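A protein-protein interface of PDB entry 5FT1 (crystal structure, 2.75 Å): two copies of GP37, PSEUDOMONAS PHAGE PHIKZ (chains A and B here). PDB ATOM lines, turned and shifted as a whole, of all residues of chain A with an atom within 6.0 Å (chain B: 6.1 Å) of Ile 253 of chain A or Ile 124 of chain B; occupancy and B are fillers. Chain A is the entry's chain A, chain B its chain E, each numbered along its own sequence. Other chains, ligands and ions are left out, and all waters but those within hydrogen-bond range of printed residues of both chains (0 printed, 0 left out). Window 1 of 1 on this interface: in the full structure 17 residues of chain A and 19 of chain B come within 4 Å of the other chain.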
ATOM      1  N   ALA A 115     -26.467  -4.700 -20.620  1.00  0.00           N
ATOM      2  CA  ALA A 115     -25.423  -4.461 -21.610  1.00  0.00           C
ATOM      3  C   ALA A 115     -25.783  -5.063 -22.964  1.00  0.00           C
ATOM      4  O   ALA A 115     -26.482  -6.071 -23.042  1.00  0.00           O
ATOM      5  CB  ALA A 115     -24.093  -5.011 -21.121  1.00  0.00           C
ATOM      6  N   ASP A 116     -25.296  -4.434 -24.028  1.00  0.00           N
ATOM      7  CA  ASP A 116     -25.552  -4.889 -25.383  1.00  0.00           C
ATOM      8  C   ASP A 116     -24.494  -5.911 -25.770  1.00  0.00           C
ATOM      9  O   ASP A 116     -24.790  -6.942 -26.373  1.00  0.00           O
ATOM     10  CB  ASP A 116     -25.535  -3.712 -26.358  1.00  0.00           C
ATOM     11  N   LEU A 249     -22.086 -10.993 -14.851  1.00  0.00           N
ATOM     12  CA  LEU A 249     -22.571 -12.093 -15.677  1.00  0.00           C
ATOM     13  C   LEU A 249     -23.701 -11.634 -16.587  1.00  0.00           C
ATOM     14  O   LEU A 249     -23.928 -12.225 -17.648  1.00  0.00           O
ATOM     15  CB  LEU A 249     -23.041 -13.256 -14.800  1.00  0.00           C
ATOM     16  CG  LEU A 249     -22.017 -14.145 -14.083  1.00  0.00           C
ATOM     17  CD1 LEU A 249     -21.375 -13.451 -12.884  1.00  0.00           C
ATOM     18  CD2 LEU A 249     -22.665 -15.457 -13.662  1.00  0.00           C
ATOM     19  N   LEU A 250     -24.419 -10.585 -16.184  1.00  0.00           N
ATOM     20  CA  LEU A 250     -25.476  -9.998 -16.992  1.00  0.00           C
ATOM     21  C   LEU A 250     -24.935  -9.130 -18.120  1.00  0.00           C
ATOM     22  O   LEU A 250     -25.714  -8.700 -18.977  1.00  0.00           O
ATOM     23  CB  LEU A 250     -26.421  -9.181 -16.104  1.00  0.00           C
ATOM     24  CG  LEU A 250     -27.254  -9.941 -15.059  1.00  0.00           C
ATOM     25  CD1 LEU A 250     -26.440 -10.327 -13.825  1.00  0.00           C
ATOM     26  CD2 LEU A 250     -28.477  -9.132 -14.657  1.00  0.00           C
ATOM     27  N   SER A 251     -23.632  -8.859 -18.137  1.00  0.00           N
ATOM     28  CA  SER A 251     -22.975  -8.248 -19.284  1.00  0.00           C
ATOM     29  C   SER A 251     -22.561  -9.277 -20.324  1.00  0.00           C
ATOM     30  O   SER A 251     -22.049  -8.900 -21.383  1.00  0.00           O
ATOM     31  CB  SER A 251     -21.749  -7.449 -18.832  1.00  0.00           C
ATOM     32  OG  SER A 251     -20.778  -8.295 -18.240  1.00  0.00           O
ATOM     33  N   HIS A 252     -22.768 -10.563 -20.044  1.00  0.00           N
ATOM     34  CA  HIS A 252     -22.430 -11.640 -20.961  1.00  0.00           C
ATOM     35  C   HIS A 252     -23.654 -12.298 -21.581  1.00  0.00           C
ATOM     36  O   HIS A 252     -23.500 -13.167 -22.445  1.00  0.00           O
ATOM     37  CB  HIS A 252     -21.593 -12.707 -20.241  1.00  0.00           C
ATOM     38  CG  HIS A 252     -20.294 -12.198 -19.699  1.00  0.00           C
ATOM     39  ND1 HIS A 252     -19.220 -11.891 -20.506  1.00  0.00           N
ATOM     40  CD2 HIS A 252     -19.892 -11.953 -18.429  1.00  0.00           C
ATOM     41  CE1 HIS A 252     -18.214 -11.474 -19.757  1.00  0.00           C
ATOM     42  NE2 HIS A 252     -18.596 -11.503 -18.493  1.00  0.00           N
ATOM     43  N   ILE A 253     -24.859 -11.915 -21.170  1.00  0.00           N
ATOM     44  CA  ILE A 253     -26.071 -12.593 -21.615  1.00  0.00           C
ATOM     45  C   ILE A 253     -26.388 -12.187 -23.047  1.00  0.00           C
ATOM     46  O   ILE A 253     -26.389 -10.997 -23.386  1.00  0.00           O
ATOM     47  CB  ILE A 253     -27.247 -12.279 -20.678  1.00  0.00           C
ATOM     48  CG1 ILE A 253     -26.894 -12.641 -19.235  1.00  0.00           C
ATOM     49  CG2 ILE A 253     -28.495 -13.028 -21.122  1.00  0.00           C
ATOM     50  CD1 ILE A 253     -28.010 -12.367 -18.250  1.00  0.00           C
ATOM     51  N   ARG A 254     -26.657 -13.176 -23.890  1.00  0.00           N
ATOM     52  CA  ARG A 254     -27.134 -12.976 -25.250  1.00  0.00           C
ATOM     53  C   ARG A 254     -28.440 -13.751 -25.428  1.00  0.00           C
ATOM     54  O   ARG A 254     -28.984 -14.317 -24.477  1.00  0.00           O
ATOM     55  CB  ARG A 254     -26.070 -13.405 -26.265  1.00  0.00           C
ATOM     56  N   THR A 255     -28.949 -13.768 -26.657  1.00  0.00           N
ATOM     57  CA  THR A 255     -30.167 -14.494 -26.984  1.00  0.00           C
ATOM     58  C   THR A 255     -29.959 -15.293 -28.262  1.00  0.00           C
ATOM     59  O   THR A 255     -29.201 -14.892 -29.150  1.00  0.00           O
ATOM     60  CB  THR A 255     -31.373 -13.556 -27.154  1.00  0.00           C
ATOM     61  OG1 THR A 255     -31.081 -12.571 -28.154  1.00  0.00           O
ATOM     62  CG2 THR A 255     -31.706 -12.862 -25.840  1.00  0.00           C
ATOM     63  N   VAL A 256     -30.645 -16.429 -28.346  1.00  0.00           N
ATOM     64  CA  VAL A 256     -30.539 -17.304 -29.505  1.00  0.00           C
ATOM     65  C   VAL A 256     -31.776 -18.189 -29.617  1.00  0.00           C
ATOM     66  O   VAL A 256     -32.657 -18.150 -28.759  1.00  0.00           O
ATOM     67  CB  VAL A 256     -29.264 -18.161 -29.439  1.00  0.00           C
ATOM     68  N   ILE B 104     -28.818 -24.887 -24.036  1.00  0.00           N
ATOM     69  CA  ILE B 104     -29.615 -24.384 -25.152  1.00  0.00           C
ATOM     70  C   ILE B 104     -28.671 -23.875 -26.230  1.00  0.00           C
ATOM     71  O   ILE B 104     -27.638 -23.269 -25.926  1.00  0.00           O
ATOM     72  CB  ILE B 104     -30.581 -23.273 -24.695  1.00  0.00           C
ATOM     73  CG1 ILE B 104     -31.458 -23.758 -23.537  1.00  0.00           C
ATOM     74  CG2 ILE B 104     -31.451 -22.807 -25.854  1.00  0.00           C
ATOM     75  CD1 ILE B 104     -30.924 -23.401 -22.161  1.00  0.00           C
ATOM     76  N   GLY B 111     -25.326 -22.687 -24.124  1.00  0.00           N
ATOM     77  CA  GLY B 111     -25.202 -22.190 -22.766  1.00  0.00           C
ATOM     78  C   GLY B 111     -26.525 -22.124 -22.031  1.00  0.00           C
ATOM     79  O   GLY B 111     -27.383 -22.988 -22.206  1.00  0.00           O
ATOM     80  N   HIS B 113     -30.684 -21.196 -19.146  1.00  0.00           N
ATOM     81  CA  HIS B 113     -30.957 -19.766 -19.087  1.00  0.00           C
ATOM     82  C   HIS B 113     -30.926 -19.151 -20.483  1.00  0.00           C
ATOM     83  O   HIS B 113     -30.029 -19.444 -21.271  1.00  0.00           O
ATOM     84  CB  HIS B 113     -29.948 -19.063 -18.177  1.00  0.00           C
ATOM     85  N   ILE B 114     -31.909 -18.308 -20.790  1.00  0.00           N
ATOM     86  CA  ILE B 114     -32.994 -18.000 -19.865  1.00  0.00           C
ATOM     87  C   ILE B 114     -34.327 -18.425 -20.468  1.00  0.00           C
ATOM     88  O   ILE B 114     -34.414 -18.721 -21.659  1.00  0.00           O
ATOM     89  CB  ILE B 114     -33.008 -16.507 -19.497  1.00  0.00           C
ATOM     90  N   ILE B 124     -29.642 -16.254 -23.456  1.00  0.00           N
ATOM     91  CA  ILE B 124     -28.700 -17.335 -23.202  1.00  0.00           C
ATOM     92  C   ILE B 124     -27.401 -16.789 -22.621  1.00  0.00           C
ATOM     93  O   ILE B 124     -26.921 -15.735 -23.035  1.00  0.00           O
ATOM     94  CB  ILE B 124     -28.423 -18.143 -24.481  1.00  0.00           C
ATOM     95  N   LEU B 125     -26.840 -17.514 -21.653  1.00  0.00           N
ATOM     96  CA  LEU B 125     -25.546 -17.160 -21.089  1.00  0.00           C
ATOM     97  C   LEU B 125     -24.488 -18.067 -21.695  1.00  0.00           C
ATOM     98  O   LEU B 125     -24.490 -19.275 -21.414  1.00  0.00           O
ATOM     99  CB  LEU B 125     -25.559 -17.292 -19.568  1.00  0.00           C
ATOM    100  CG  LEU B 125     -24.274 -16.860 -18.860  1.00  0.00           C
ATOM    101  CD1 LEU B 125     -23.951 -15.407 -19.177  1.00  0.00           C
ATOM    102  CD2 LEU B 125     -24.389 -17.070 -17.359  1.00  0.00           C
ATOM    103  N   PRO B 126     -23.594 -17.548 -22.537  1.00  0.00           N
ATOM    104  CA  PRO B 126     -22.608 -18.407 -23.202  1.00  0.00           C
ATOM    105  C   PRO B 126     -21.800 -19.241 -22.219  1.00  0.00           C
ATOM    106  O   PRO B 126     -21.398 -18.772 -21.151  1.00  0.00           O
ATOM    107  CB  PRO B 126     -21.711 -17.410 -23.945  1.00  0.00           C
ATOM    108  CG  PRO B 126     -22.494 -16.148 -24.054  1.00  0.00           C
ATOM    109  CD  PRO B 126     -23.709 -16.228 -23.177  1.00  0.00           C
ATOM    110  N   PHE B 244     -28.237 -16.083  -7.350  1.00  0.00           N
ATOM    111  CA  PHE B 244     -28.342 -15.201  -8.506  1.00  0.00           C
ATOM    112  C   PHE B 244     -29.239 -15.791  -9.590  1.00  0.00           C
ATOM    113  O   PHE B 244     -30.097 -15.091 -10.139  1.00  0.00           O
ATOM    114  CB  PHE B 244     -26.946 -14.910  -9.069  1.00  0.00           C
ATOM    115  CG  PHE B 244     -26.905 -14.796 -10.568  1.00  0.00           C
ATOM    116  CD1 PHE B 244     -27.314 -13.634 -11.199  1.00  0.00           C
ATOM    117  CD2 PHE B 244     -26.445 -15.848 -11.345  1.00  0.00           C
ATOM    118  CE1 PHE B 244     -27.277 -13.527 -12.577  1.00  0.00           C
ATOM    119  CE2 PHE B 244     -26.405 -15.746 -12.722  1.00  0.00           C
ATOM    120  CZ  PHE B 244     -26.821 -14.583 -13.339  1.00  0.00           C
ATOM    121  N   LEU B 250     -34.425 -12.810 -14.002  1.00  0.00           N
ATOM    122  CA  LEU B 250     -34.089 -13.658 -15.137  1.00  0.00           C
ATOM    123  C   LEU B 250     -35.361 -14.352 -15.608  1.00  0.00           C
ATOM    124  O   LEU B 250     -36.000 -15.061 -14.824  1.00  0.00           O
ATOM    125  CB  LEU B 250     -33.040 -14.688 -14.734  1.00  0.00           C
ATOM    126  CG  LEU B 250     -31.948 -14.222 -13.772  1.00  0.00           C
ATOM    127  CD1 LEU B 250     -31.119 -15.402 -13.338  1.00  0.00           C
ATOM    128  CD2 LEU B 250     -31.062 -13.173 -14.407  1.00  0.00           C
ATOM    129  N   ILE B 253     -36.169 -10.245 -18.668  1.00  0.00           N
ATOM    130  CA  ILE B 253     -35.334  -9.343 -19.451  1.00  0.00           C
ATOM    131  C   ILE B 253     -35.312  -9.811 -20.899  1.00  0.00           C
ATOM    132  O   ILE B 253     -35.157 -11.007 -21.174  1.00  0.00           O
ATOM    133  CB  ILE B 253     -33.904  -9.259 -18.890  1.00  0.00           C
ATOM    134  CG1 ILE B 253     -33.409 -10.642 -18.463  1.00  0.00           C
ATOM    135  CG2 ILE B 253     -33.835  -8.270 -17.741  1.00  0.00           C
ATOM    136  CD1 ILE B 253     -31.996 -10.642 -17.922  1.00  0.00           C
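Positions printed for both chains: 250 and 253.
Of the 8 pairs that touch across the chains among the printed residues, none has its exchanged pair printed and touching as well.
Asp 116 of chain A touches none of the printed residues of chain B.
Of the printed residues of chain B, Leu 249 of chain A touches Leu 125 and Phe 244.
Ser 251 of chain A touches none of the printed residues of chain B.
Of chain B, only Ile 124 (3.6 Å) comes within 4 Å of Ile 253 of chain A.
Of chain A, only Ile 253, Arg 254 and Thr 255 come within 4 Å of Ile 124 of chain B.
Printed residues of chain A within 4 Å of Leu 125 of chain B: Leu 249 (3.5 Å) and His 252 (3.7 Å).
Printed residues of chain A within 4 Å of Pro 126 of chain B: His 252.
The nearest residue of chain A that does not touch Ile 124 of chain B is His 252 of chain A (4.3 Å).
N of Arg 254 of chain A is in hydrogen-bond range of O of Ile 124 of chain B, 2.7 Å away.
Of the 10 printed residues of chain B, 4 touch a printed residue of chain A.
Hydrophobic or aromatic side chains of chain B within 4 Å of the printed part of chain A: Ile 124, Leu 125, Pro 126 and Phe 244.
Of the 10 printed residues of chain A, 6 touch a printed residue of chain B.
Printed residues of chain A that touch a printed residue of chain B: Leu 249, Leu 250, His 252, Ile 253, Arg 254 and Thr 255.
Hydrophobic or aromatic side chains of chain A that line the printed part of chain B: Leu 249, Leu 250, His 252 and Ile 253.
Among the printed residues, 8 pairs touch across the chains.
Among the printed residues, no Asp or Glu carboxylate lies within 4 Å of a Lys or Arg side-chain nitrogen of the other chain.
Among the printed residues, merely in contact across the chains: His 252 of chain A with Pro 126 of chain B, Leu 249 of chain A with Leu 125 of chain B, Leu 250 of chain A with Phe 244 of chain B, Ile 253 of chain A with Ile 124 of chain B, His 252 of chain A with Leu 125 of chain B, Leu 249 of chain A with Phe 244 of chain B and Thr 255 of chain A with Ile 124 of chain B.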
